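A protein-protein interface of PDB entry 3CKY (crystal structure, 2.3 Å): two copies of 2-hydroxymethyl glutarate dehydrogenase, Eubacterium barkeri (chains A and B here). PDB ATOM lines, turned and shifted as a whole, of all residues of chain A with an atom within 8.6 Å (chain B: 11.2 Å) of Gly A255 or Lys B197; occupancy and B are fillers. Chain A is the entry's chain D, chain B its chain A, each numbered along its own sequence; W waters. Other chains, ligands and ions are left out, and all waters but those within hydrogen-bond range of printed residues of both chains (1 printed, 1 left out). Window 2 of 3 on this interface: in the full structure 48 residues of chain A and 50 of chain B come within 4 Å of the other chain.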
ATOM      1  N   PRO A 102      13.922  23.912  14.900  1.00  0.00           N
ATOM      2  CA  PRO A 102      14.117  23.747  16.348  1.00  0.00           C
ATOM      3  C   PRO A 102      15.080  22.614  16.714  1.00  0.00           C
ATOM      4  O   PRO A 102      15.910  22.785  17.601  1.00  0.00           O
ATOM      5  CB  PRO A 102      12.711  23.425  16.864  1.00  0.00           C
ATOM      6  CG  PRO A 102      11.783  24.004  15.869  1.00  0.00           C
ATOM      7  CD  PRO A 102      12.493  23.952  14.536  1.00  0.00           C
ATOM      8  N   ALA A 172      10.378  27.443  16.170  1.00  0.00           N
ATOM      9  CA  ALA A 172       9.026  26.970  15.871  1.00  0.00           C
ATOM     10  C   ALA A 172       8.082  28.114  15.497  1.00  0.00           C
ATOM     11  O   ALA A 172       7.374  28.029  14.493  1.00  0.00           O
ATOM     12  CB  ALA A 172       8.470  26.178  17.075  1.00  0.00           C
ATOM     13  N   VAL A 176       6.155  28.894  11.976  1.00  0.00           N
ATOM     14  CA  VAL A 176       4.693  28.911  11.871  1.00  0.00           C
ATOM     15  C   VAL A 176       4.186  30.256  11.312  1.00  0.00           C
ATOM     16  O   VAL A 176       3.300  30.281  10.452  1.00  0.00           O
ATOM     17  CB  VAL A 176       4.043  28.592  13.219  1.00  0.00           C
ATOM     18  CG1 VAL A 176       2.520  28.770  13.148  1.00  0.00           C
ATOM     19  CG2 VAL A 176       4.407  27.194  13.635  1.00  0.00           C
ATOM     20  N   ALA A 248       9.208  24.721   7.289  1.00  0.00           N
ATOM     21  CA  ALA A 248       7.915  24.261   7.806  1.00  0.00           C
ATOM     22  C   ALA A 248       7.676  22.784   7.442  1.00  0.00           C
ATOM     23  O   ALA A 248       7.326  21.959   8.310  1.00  0.00           O
ATOM     24  CB  ALA A 248       6.777  25.142   7.285  1.00  0.00           C
ATOM     25  N   LEU A 249       7.915  22.437   6.185  1.00  0.00           N
ATOM     26  CA  LEU A 249       7.728  21.056   5.726  1.00  0.00           C
ATOM     27  C   LEU A 249       8.689  20.097   6.431  1.00  0.00           C
ATOM     28  O   LEU A 249       8.319  18.948   6.755  1.00  0.00           O
ATOM     29  CB  LEU A 249       7.893  20.958   4.212  1.00  0.00           C
ATOM     30  CG  LEU A 249       6.856  21.714   3.372  1.00  0.00           C
ATOM     31  CD1 LEU A 249       7.244  21.637   1.875  1.00  0.00           C
ATOM     32  CD2 LEU A 249       5.430  21.183   3.570  1.00  0.00           C
ATOM     33  N   GLU A 250       9.911  20.569   6.680  1.00  0.00           N
ATOM     34  CA  GLU A 250      10.879  19.790   7.452  1.00  0.00           C
ATOM     35  C   GLU A 250      10.343  19.527   8.867  1.00  0.00           C
ATOM     36  O   GLU A 250      10.419  18.397   9.371  1.00  0.00           O
ATOM     37  CB  GLU A 250      12.247  20.507   7.517  1.00  0.00           C
ATOM     38  CG  GLU A 250      13.325  19.675   8.203  1.00  0.00           C
ATOM     39  CD  GLU A 250      14.567  20.461   8.669  1.00  0.00           C
ATOM     40  OE1 GLU A 250      15.379  19.841   9.403  1.00  0.00           O
ATOM     41  OE2 GLU A 250      14.735  21.666   8.337  1.00  0.00           O
ATOM     42  N   ALA A 251       9.813  20.574   9.501  1.00  0.00           N
ATOM     43  CA  ALA A 251       9.215  20.447  10.841  1.00  0.00           C
ATOM     44  C   ALA A 251       7.972  19.528  10.827  1.00  0.00           C
ATOM     45  O   ALA A 251       7.767  18.729  11.733  1.00  0.00           O
ATOM     46  CB  ALA A 251       8.877  21.824  11.418  1.00  0.00           C
ATOM     47  N   GLY A 252       7.159  19.634   9.777  1.00  0.00           N
ATOM     48  CA  GLY A 252       6.004  18.740   9.609  1.00  0.00           C
ATOM     49  C   GLY A 252       6.381  17.278   9.487  1.00  0.00           C
ATOM     50  O   GLY A 252       5.752  16.422  10.100  1.00  0.00           O
ATOM     51  N   LYS A 253       7.422  16.992   8.708  1.00  0.00           N
ATOM     52  CA  LYS A 253       7.956  15.635   8.569  1.00  0.00           C
ATOM     53  C   LYS A 253       8.510  15.090   9.894  1.00  0.00           C
ATOM     54  O   LYS A 253       8.260  13.929  10.260  1.00  0.00           O
ATOM     55  CB  LYS A 253       9.055  15.600   7.487  1.00  0.00           C
ATOM     56  CG  LYS A 253       9.878  14.310   7.443  1.00  0.00           C
ATOM     57  CD  LYS A 253      10.715  14.189   6.161  1.00  0.00           C
ATOM     58  CE  LYS A 253      11.386  12.787   6.049  1.00  0.00           C
ATOM     59  NZ  LYS A 253      11.978  12.482   4.665  1.00  0.00           N
ATOM     60  N   GLU A 254       9.282  15.917  10.589  1.00  0.00           N
ATOM     61  CA  GLU A 254       9.887  15.523  11.863  1.00  0.00           C
ATOM     62  C   GLU A 254       8.832  15.317  12.938  1.00  0.00           C
ATOM     63  O   GLU A 254       8.999  14.460  13.785  1.00  0.00           O
ATOM     64  CB  GLU A 254      10.922  16.560  12.319  1.00  0.00           C
ATOM     65  CG  GLU A 254      12.170  16.607  11.417  1.00  0.00           C
ATOM     66  CD  GLU A 254      13.037  17.861  11.607  1.00  0.00           C
ATOM     67  OE1 GLU A 254      12.549  18.865  12.182  1.00  0.00           O
ATOM     68  OE2 GLU A 254      14.213  17.849  11.163  1.00  0.00           O
ATOM     69  N   GLY A 255       7.743  16.082  12.895  1.00  0.00           N
ATOM     70  CA  GLY A 255       6.677  15.962  13.898  1.00  0.00           C
ATOM     71  C   GLY A 255       5.468  15.138  13.473  1.00  0.00           C
ATOM     72  O   GLY A 255       4.502  15.039  14.201  1.00  0.00           O
ATOM     73  N   ASN A 256       5.523  14.557  12.281  1.00  0.00           N
ATOM     74  CA  ASN A 256       4.385  13.850  11.692  1.00  0.00           C
ATOM     75  C   ASN A 256       3.088  14.666  11.688  1.00  0.00           C
ATOM     76  O   ASN A 256       2.043  14.205  12.133  1.00  0.00           O
ATOM     77  CB  ASN A 256       4.168  12.497  12.377  1.00  0.00           C
ATOM     78  CG  ASN A 256       5.405  11.611  12.322  1.00  0.00           C
ATOM     79  OD1 ASN A 256       5.887  11.251  11.241  1.00  0.00           O
ATOM     80  ND2 ASN A 256       5.927  11.265  13.487  1.00  0.00           N
ATOM     81  N   VAL A 257       3.187  15.885  11.165  1.00  0.00           N
ATOM     82  CA  VAL A 257       2.046  16.773  11.017  1.00  0.00           C
ATOM     83  C   VAL A 257       1.894  17.069   9.523  1.00  0.00           C
ATOM     84  O   VAL A 257       2.769  17.672   8.911  1.00  0.00           O
ATOM     85  CB  VAL A 257       2.254  18.079  11.796  1.00  0.00           C
ATOM     86  CG1 VAL A 257       1.119  19.073  11.519  1.00  0.00           C
ATOM     87  CG2 VAL A 257       2.438  17.779  13.325  1.00  0.00           C
ATOM     88  N   PRO A 258       0.808  16.584   8.913  1.00  0.00           N
ATOM     89  CA  PRO A 258       0.536  16.940   7.524  1.00  0.00           C
ATOM     90  C   PRO A 258       0.335  18.443   7.314  1.00  0.00           C
ATOM     91  O   PRO A 258      -0.307  19.109   8.125  1.00  0.00           O
ATOM     92  CB  PRO A 258      -0.767  16.179   7.212  1.00  0.00           C
ATOM     93  CG  PRO A 258      -0.836  15.087   8.244  1.00  0.00           C
ATOM     94  CD  PRO A 258      -0.195  15.648   9.458  1.00  0.00           C
ATOM     95  N   LEU A 259       0.862  18.950   6.208  1.00  0.00           N
ATOM     96  CA  LEU A 259       0.867  20.367   5.879  1.00  0.00           C
ATOM     97  C   LEU A 259       0.508  20.526   4.396  1.00  0.00           C
ATOM     98  O   LEU A 259       1.313  20.991   3.587  1.00  0.00           O
ATOM     99  CB  LEU A 259       2.245  20.962   6.164  1.00  0.00           C
ATOM    100  CG  LEU A 259       2.747  20.998   7.617  1.00  0.00           C
ATOM    101  CD1 LEU A 259       4.236  21.427   7.638  1.00  0.00           C
ATOM    102  CD2 LEU A 259       1.893  21.913   8.495  1.00  0.00           C
ATOM    103  N   LEU B 188      -4.253  28.140   8.517  1.00  0.00           N
ATOM    104  CA  LEU B 188      -4.161  28.334   9.967  1.00  0.00           C
ATOM    105  C   LEU B 188      -4.298  27.006  10.727  1.00  0.00           C
ATOM    106  O   LEU B 188      -3.544  26.724  11.676  1.00  0.00           O
ATOM    107  CB  LEU B 188      -5.232  29.332  10.431  1.00  0.00           C
ATOM    108  CG  LEU B 188      -5.167  29.760  11.907  1.00  0.00           C
ATOM    109  CD1 LEU B 188      -3.815  30.435  12.248  1.00  0.00           C
ATOM    110  CD2 LEU B 188      -6.351  30.645  12.263  1.00  0.00           C
ATOM    111  N   ALA B 189      -5.240  26.185  10.285  1.00  0.00           N
ATOM    112  CA  ALA B 189      -5.514  24.901  10.932  1.00  0.00           C
ATOM    113  C   ALA B 189      -4.252  24.032  11.089  1.00  0.00           C
ATOM    114  O   ALA B 189      -3.904  23.613  12.217  1.00  0.00           O
ATOM    115  CB  ALA B 189      -6.586  24.149  10.159  1.00  0.00           C
ATOM    116  N   GLU B 190      -3.580  23.766   9.959  1.00  0.00           N
ATOM    117  CA  GLU B 190      -2.374  22.935   9.967  1.00  0.00           C
ATOM    118  C   GLU B 190      -1.204  23.630  10.680  1.00  0.00           C
ATOM    119  O   GLU B 190      -0.413  22.971  11.373  1.00  0.00           O
ATOM    120  CB  GLU B 190      -1.992  22.495   8.552  1.00  0.00           C
ATOM    121  CG  GLU B 190      -1.471  23.618   7.634  1.00  0.00           C
ATOM    122  CD  GLU B 190      -1.279  23.176   6.191  1.00  0.00           C
ATOM    123  OE1 GLU B 190      -0.194  23.426   5.606  1.00  0.00           O
ATOM    124  OE2 GLU B 190      -2.226  22.586   5.632  1.00  0.00           O
ATOM    125  N   ALA B 191      -1.117  24.954  10.527  1.00  0.00           N
ATOM    126  CA  ALA B 191      -0.076  25.761  11.183  1.00  0.00           C
ATOM    127  C   ALA B 191      -0.109  25.672  12.700  1.00  0.00           C
ATOM    128  O   ALA B 191       0.936  25.557  13.359  1.00  0.00           O
ATOM    129  CB  ALA B 191      -0.192  27.223  10.761  1.00  0.00           C
ATOM    130  N   LEU B 192      -1.309  25.758  13.261  1.00  0.00           N
ATOM    131  CA  LEU B 192      -1.485  25.715  14.709  1.00  0.00           C
ATOM    132  C   LEU B 192      -1.150  24.339  15.277  1.00  0.00           C
ATOM    133  O   LEU B 192      -0.516  24.221  16.320  1.00  0.00           O
ATOM    134  CB  LEU B 192      -2.909  26.116  15.080  1.00  0.00           C
ATOM    135  CG  LEU B 192      -3.271  27.593  14.871  1.00  0.00           C
ATOM    136  CD1 LEU B 192      -4.743  27.823  15.223  1.00  0.00           C
ATOM    137  CD2 LEU B 192      -2.366  28.503  15.701  1.00  0.00           C
ATOM    138  N   VAL B 193      -1.561  23.301  14.566  1.00  0.00           N
ATOM    139  CA  VAL B 193      -1.228  21.934  14.942  1.00  0.00           C
ATOM    140  C   VAL B 193       0.292  21.700  14.934  1.00  0.00           C
ATOM    141  O   VAL B 193       0.830  21.079  15.861  1.00  0.00           O
ATOM    142  CB  VAL B 193      -1.940  20.939  14.008  1.00  0.00           C
ATOM    143  CG1 VAL B 193      -1.427  19.507  14.223  1.00  0.00           C
ATOM    144  CG2 VAL B 193      -3.468  21.063  14.176  1.00  0.00           C
ATOM    145  N   LEU B 194       0.965  22.200  13.890  1.00  0.00           N
ATOM    146  CA  LEU B 194       2.421  22.134  13.790  1.00  0.00           C
ATOM    147  C   LEU B 194       3.093  22.807  14.983  1.00  0.00           C
ATOM    148  O   LEU B 194       3.996  22.237  15.585  1.00  0.00           O
ATOM    149  CB  LEU B 194       2.899  22.799  12.498  1.00  0.00           C
ATOM    150  CG  LEU B 194       4.425  22.790  12.210  1.00  0.00           C
ATOM    151  CD1 LEU B 194       4.979  21.367  12.066  1.00  0.00           C
ATOM    152  CD2 LEU B 194       4.785  23.639  11.001  1.00  0.00           C
ATOM    153  N   GLY B 195       2.632  24.017  15.301  1.00  0.00           N
ATOM    154  CA  GLY B 195       3.177  24.814  16.391  1.00  0.00           C
ATOM    155  C   GLY B 195       3.070  24.108  17.712  1.00  0.00           C
ATOM    156  O   GLY B 195       4.048  24.047  18.442  1.00  0.00           O
ATOM    157  N   VAL B 196       1.887  23.564  18.001  1.00  0.00           N
ATOM    158  CA  VAL B 196       1.671  22.816  19.233  1.00  0.00           C
ATOM    159  C   VAL B 196       2.602  21.614  19.272  1.00  0.00           C
ATOM    160  O   VAL B 196       3.303  21.395  20.246  1.00  0.00           O
ATOM    161  CB  VAL B 196       0.189  22.397  19.438  1.00  0.00           C
ATOM    162  CG1 VAL B 196       0.061  21.424  20.642  1.00  0.00           C
ATOM    163  CG2 VAL B 196      -0.683  23.646  19.648  1.00  0.00           C
ATOM    164  N   LYS B 197       2.649  20.864  18.180  1.00  0.00           N
ATOM    165  CA  LYS B 197       3.551  19.720  18.102  1.00  0.00           C
ATOM    166  C   LYS B 197       5.021  20.103  18.367  1.00  0.00           C
ATOM    167  O   LYS B 197       5.771  19.316  18.954  1.00  0.00           O
ATOM    168  CB  LYS B 197       3.435  19.047  16.741  1.00  0.00           C
ATOM    169  CG  LYS B 197       4.248  17.768  16.617  1.00  0.00           C
ATOM    170  CD  LYS B 197       3.605  16.648  17.432  1.00  0.00           C
ATOM    171  CE  LYS B 197       4.425  15.371  17.403  1.00  0.00           C
ATOM    172  NZ  LYS B 197       3.524  14.203  17.141  1.00  0.00           N
ATOM    173  N   CYS B 198       5.418  21.303  17.931  1.00  0.00           N
ATOM    174  CA  CYS B 198       6.750  21.842  18.227  1.00  0.00           C
ATOM    175  C   CYS B 198       6.864  22.526  19.602  1.00  0.00           C
ATOM    176  O   CYS B 198       7.867  23.165  19.868  1.00  0.00           O
ATOM    177  CB  CYS B 198       7.165  22.851  17.160  1.00  0.00           C
ATOM    178  SG  CYS B 198       7.244  22.222  15.455  1.00  0.00           S
ATOM    179  N   GLY B 199       5.840  22.417  20.450  1.00  0.00           N
ATOM    180  CA  GLY B 199       5.917  22.865  21.844  1.00  0.00           C
ATOM    181  C   GLY B 199       5.459  24.275  22.097  1.00  0.00           C
ATOM    182  O   GLY B 199       5.758  24.821  23.141  1.00  0.00           O
ATOM    183  N   LEU B 200       4.731  24.866  21.159  1.00  0.00           N
ATOM    184  CA  LEU B 200       4.150  26.195  21.354  1.00  0.00           C
ATOM    185  C   LEU B 200       2.762  26.063  21.941  1.00  0.00           C
ATOM    186  O   LEU B 200       1.994  25.189  21.554  1.00  0.00           O
ATOM    187  CB  LEU B 200       4.030  26.950  20.024  1.00  0.00           C
ATOM    188  CG  LEU B 200       5.348  27.224  19.303  1.00  0.00           C
ATOM    189  CD1 LEU B 200       5.093  27.809  17.928  1.00  0.00           C
ATOM    190  CD2 LEU B 200       6.266  28.140  20.121  1.00  0.00           C
ATOM    191  N   LYS B 201       2.457  26.960  22.858  1.00  0.00           N
ATOM    192  CA  LYS B 201       1.107  27.107  23.373  1.00  0.00           C
ATOM    193  C   LYS B 201       0.330  27.925  22.363  1.00  0.00           C
ATOM    194  O   LYS B 201       0.901  28.827  21.733  1.00  0.00           O
ATOM    195  CB  LYS B 201       1.163  27.810  24.733  1.00  0.00           C
ATOM    196  CG  LYS B 201       1.863  26.959  25.773  1.00  0.00           C
ATOM    197  CD  LYS B 201       2.966  27.680  26.553  1.00  0.00           C
ATOM    198  CE  LYS B 201       2.435  28.671  27.549  1.00  0.00           C
ATOM    199  NZ  LYS B 201       3.395  28.891  28.708  1.00  0.00           N
ATOM    200  N   PRO B 202      -0.966  27.611  22.176  1.00  0.00           N
ATOM    201  CA  PRO B 202      -1.836  28.438  21.326  1.00  0.00           C
ATOM    202  C   PRO B 202      -1.794  29.925  21.679  1.00  0.00           C
ATOM    203  O   PRO B 202      -1.828  30.766  20.780  1.00  0.00           O
ATOM    204  CB  PRO B 202      -3.230  27.855  21.583  1.00  0.00           C
ATOM    205  CG  PRO B 202      -2.980  26.460  21.977  1.00  0.00           C
ATOM    206  CD  PRO B 202      -1.686  26.453  22.728  1.00  0.00           C
ATOM    207  N   MET B 205       1.262  31.553  20.200  1.00  0.00           N
ATOM    208  CA  MET B 205       1.045  31.754  18.776  1.00  0.00           C
ATOM    209  C   MET B 205       0.071  32.884  18.484  1.00  0.00           C
ATOM    210  O   MET B 205       0.320  33.701  17.614  1.00  0.00           O
ATOM    211  CB  MET B 205       0.578  30.457  18.110  1.00  0.00           C
ATOM    212  CG  MET B 205       1.702  29.442  17.936  1.00  0.00           C
ATOM    213  SD  MET B 205       1.211  27.956  17.015  1.00  0.00           S
ATOM    214  CE  MET B 205       0.161  27.112  18.203  1.00  0.00           C
ATOM    215  N   ILE B 286      -9.883  22.360  11.977  1.00  0.00           N
ATOM    216  CA  ILE B 286      -8.682  21.997  12.722  1.00  0.00           C
ATOM    217  C   ILE B 286      -8.773  20.573  13.345  1.00  0.00           C
ATOM    218  O   ILE B 286      -7.770  19.866  13.455  1.00  0.00           O
ATOM    219  CB  ILE B 286      -8.325  23.048  13.831  1.00  0.00           C
ATOM    220  CG1 ILE B 286      -6.868  22.878  14.278  1.00  0.00           C
ATOM    221  CG2 ILE B 286      -9.260  22.913  15.058  1.00  0.00           C
ATOM    222  CD1 ILE B 286      -6.309  24.022  15.127  1.00  0.00           C
ATOM    223  N   TRP B 289      -7.041  17.562  11.669  1.00  0.00           N
ATOM    224  CA  TRP B 289      -5.637  17.283  11.944  1.00  0.00           C
ATOM    225  C   TRP B 289      -5.402  16.772  13.364  1.00  0.00           C
ATOM    226  O   TRP B 289      -4.551  15.915  13.584  1.00  0.00           O
ATOM    227  CB  TRP B 289      -4.796  18.533  11.660  1.00  0.00           C
ATOM    228  CG  TRP B 289      -4.935  19.046  10.242  1.00  0.00           C
ATOM    229  CD1 TRP B 289      -5.222  20.316   9.870  1.00  0.00           C
ATOM    230  CD2 TRP B 289      -4.823  18.283   9.017  1.00  0.00           C
ATOM    231  NE1 TRP B 289      -5.286  20.409   8.496  1.00  0.00           N
ATOM    232  CE2 TRP B 289      -5.049  19.175   7.950  1.00  0.00           C
ATOM    233  CE3 TRP B 289      -4.565  16.931   8.726  1.00  0.00           C
ATOM    234  CZ2 TRP B 289      -5.016  18.768   6.604  1.00  0.00           C
ATOM    235  CZ3 TRP B 289      -4.539  16.527   7.393  1.00  0.00           C
ATOM    236  CH2 TRP B 289      -4.758  17.449   6.349  1.00  0.00           C
ATOM    237  N   GLU B 290      -6.176  17.290  14.318  1.00  0.00           N
ATOM    238  CA  GLU B 290      -6.131  16.828  15.714  1.00  0.00           C
ATOM    239  C   GLU B 290      -6.470  15.359  15.806  1.00  0.00           C
ATOM    240  O   GLU B 290      -5.804  14.609  16.513  1.00  0.00           O
ATOM    241  CB  GLU B 290      -7.088  17.640  16.600  1.00  0.00           C
ATOM    242  CG  GLU B 290      -6.682  19.098  16.702  1.00  0.00           C
ATOM    243  CD  GLU B 290      -7.607  19.928  17.563  1.00  0.00           C
ATOM    244  OE1 GLU B 290      -7.075  20.656  18.443  1.00  0.00           O
ATOM    245  OE2 GLU B 290      -8.843  19.858  17.362  1.00  0.00           O
ATOM    246  N   GLN B 291      -7.500  14.952  15.084  1.00  0.00           N
ATOM    247  CA  GLN B 291      -7.924  13.573  15.128  1.00  0.00           C
ATOM    248  C   GLN B 291      -6.849  12.685  14.483  1.00  0.00           C
ATOM    249  O   GLN B 291      -6.562  11.602  14.982  1.00  0.00           O
ATOM    250  CB  GLN B 291      -9.283  13.397  14.439  1.00  0.00           C
ATOM    251  CG  GLN B 291      -9.793  11.954  14.385  1.00  0.00           C
ATOM    252  CD  GLN B 291      -9.864  11.282  15.755  1.00  0.00           C
ATOM    253  OE1 GLN B 291     -10.406  11.850  16.711  1.00  0.00           O
ATOM    254  NE2 GLN B 291      -9.324  10.059  15.853  1.00  0.00           N
ATOM    255  N   MET B 292      -6.256  13.150  13.392  1.00  0.00           N
ATOM    256  CA  MET B 292      -5.270  12.352  12.670  1.00  0.00           C
ATOM    257  C   MET B 292      -3.936  12.228  13.417  1.00  0.00           C
ATOM    258  O   MET B 292      -3.265  11.199  13.308  1.00  0.00           O
ATOM    259  CB  MET B 292      -5.021  12.963  11.291  1.00  0.00           C
ATOM    260  CG  MET B 292      -4.409  12.012  10.281  1.00  0.00           C
ATOM    261  SD  MET B 292      -4.148  12.813   8.698  1.00  0.00           S
ATOM    262  CE  MET B 292      -5.835  13.148   8.160  1.00  0.00           C
ATOM    263  N   THR B 293      -3.572  13.264  14.181  1.00  0.00           N
ATOM    264  CA  THR B 293      -2.230  13.383  14.773  1.00  0.00           C
ATOM    265  C   THR B 293      -2.159  13.088  16.280  1.00  0.00           C
ATOM    266  O   THR B 293      -1.087  12.774  16.797  1.00  0.00           O
ATOM    267  CB  THR B 293      -1.630  14.829  14.531  1.00  0.00           C
ATOM    268  OG1 THR B 293      -2.426  15.833  15.191  1.00  0.00           O
ATOM    269  CG2 THR B 293      -1.498  15.134  13.028  1.00  0.00           C
ATOM    270  N   GLY B 294      -3.308  13.203  16.968  1.00  0.00           N
ATOM    271  CA  GLY B 294      -3.358  13.193  18.403  1.00  0.00           C
ATOM    272  C   GLY B 294      -2.926  14.503  19.018  1.00  0.00           C
ATOM    273  O   GLY B 294      -2.835  14.612  20.221  1.00  0.00           O
ATOM    274  N   VAL B 295      -2.646  15.508  18.202  1.00  0.00           N
ATOM    275  CA  VAL B 295      -2.247  16.813  18.730  1.00  0.00           C
ATOM    276  C   VAL B 295      -3.495  17.572  19.172  1.00  0.00           C
ATOM    277  O   VAL B 295      -4.526  17.581  18.474  1.00  0.00           O
ATOM    278  CB  VAL B 295      -1.430  17.635  17.701  1.00  0.00           C
ATOM    279  CG1 VAL B 295      -1.190  19.044  18.207  1.00  0.00           C
ATOM    280  CG2 VAL B 295      -0.103  16.931  17.406  1.00  0.00           C
ATOM    281  N   SER B 296      -3.404  18.162  20.359  1.00  0.00           N
ATOM    282  CA  SER B 296      -4.499  18.950  20.911  1.00  0.00           C
ATOM    283  C   SER B 296      -4.174  20.438  20.830  1.00  0.00           C
ATOM    284  O   SER B 296      -3.189  20.894  21.403  1.00  0.00           O
ATOM    285  CB  SER B 296      -4.774  18.566  22.367  1.00  0.00           C
ATOM    286  OG  SER B 296      -5.816  19.385  22.879  1.00  0.00           O
ATOM    287  N   VAL B 297      -4.997  21.165  20.081  1.00  0.00           N
ATOM    288  CA  VAL B 297      -4.901  22.610  19.971  1.00  0.00           C
ATOM    289  C   VAL B 297      -6.154  23.227  20.588  1.00  0.00           C
ATOM    290  O   VAL B 297      -6.070  24.076  21.491  1.00  0.00           O
ATOM    291  CB  VAL B 297      -4.773  23.075  18.491  1.00  0.00           C
ATOM    292  CG1 VAL B 297      -4.607  24.594  18.419  1.00  0.00           C
ATOM    293  CG2 VAL B 297      -3.616  22.378  17.799  1.00  0.00           C
ATOM    294  N   SER B 298      -7.316  22.803  20.091  1.00  0.00           N
ATOM    295  CA  SER B 298      -8.578  23.421  20.492  1.00  0.00           C
ATOM    296  C   SER B 298      -8.852  23.087  21.937  1.00  0.00           C
ATOM    297  O   SER B 298      -8.519  22.002  22.392  1.00  0.00           O
ATOM    298  CB  SER B 298      -9.756  22.995  19.582  1.00  0.00           C
ATOM    299  OG  SER B 298     -10.099  21.616  19.707  1.00  0.00           O
HETATM  300  O   HOH W   1       5.503  12.246  16.242  1.00  0.00           O
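The backbone carbonyl oxygen of Gly A255 lies within hydrogen-bond range of the side-chain amino group of Lys B197 (3.2 Å).
The side-chain sulfur (SG) of Cys B198 sits at hydrogen-bond distance from the backbone carbonyl oxygen (O) of Leu B194, 3.3 Å away. The backbone NH (N) of Leu B200 sits at hydrogen-bond distance from the backbone carbonyl oxygen (O) of Gly B195, at 2.9 Å. The backbone carbonyl oxygen of Trp B289 lies within hydrogen-bond range of the side-chain hydroxyl of Thr B293. The side-chain hydroxyl (OG1) of Thr B293 sits at hydrogen-bond distance from the backbone NH (N) of Val B295, at 3.0 Å. O of Gly A252 lies within hydrogen-bond range of N of Val A257 (2.8 Å).
O of Ala B191 touches CG1 of Val A176, 3.6 Å away. Gly B195 touches Val A176 (CA to CG2, 3.8 Å). Leu B194 touches Gly A252 (CD1 to N, 3.6 Å). Asn A256 touches Thr B293 (O to CG2, 3.8 Å). CG1 of Val A257 touches CG1 of Val B193, at 3.7 Å. Lys B197 touches Val A257 (CG to CG2, 3.8 Å). Glu B190 touches Pro A258. Trp B289 touches Pro A258. CD of Pro A258 touches CG2 of Thr B293, at 3.8 Å. Leu A259 touches Glu B190 (C to OE1, 3.2 Å).
Gly A255 touches just one residue of chain B: Lys B197 (3.2 Å). Of chain B, only Thr B293 (3.8 Å) comes within 4 Å of Asn A256. Of chain B, only Val B193, Leu B194 and Lys B197 come within 4 Å of Val A257. Printed residues of chain A within 4 Å of Gly B195: Val A176 (3.8 Å). Cys B198 touches just one residue of chain A: Ala A172 (3.6 Å). Of the printed residues of chain A, Leu B200 touches Ala A172 (3.8 Å). Of the printed residues of chain A, Val B193 touches Val A257. Printed residues of chain B within 4 Å of Leu A259: Glu B190. Of the printed residues of chain A, Ala B191 touches Val A176 (3.6 Å). Of the printed residues of chain B, Val A176 touches Ala B191 and Gly B195. Val B196 touches none of the printed residues of chain A. The nearest residue of chain A that does not touch Lys B197 is Asn A256 (5.1 Å).
Of the 15 printed residues of chain A, 9 touch a printed residue of chain B. Printed residues of chain A that touch a printed residue of chain B: Ala A172, Val A176, Ala A251, Gly A252, Gly A255, Asn A256, Val A257, Pro A258 and Leu A259. Hydrophobic or aromatic side chains of chain A that line the printed part of chain B: Ala A172, Val A176, Ala A251, Val A257, Pro A258 and Leu A259. Along chain A the printed residues that touch a printed residue of chain B span positions 172 to 259. Among the printed residues, no Asp or Glu carboxylate lies within 4 Å of a Lys or Arg side-chain nitrogen of the other chain.
No position is printed for both chains. Of the 15 pairs that touch across the chains among the printed residues, none has its exchanged pair printed and touching as well.
Water W1 bridges NZ of Lys B197 and ND2 of Asn A256.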
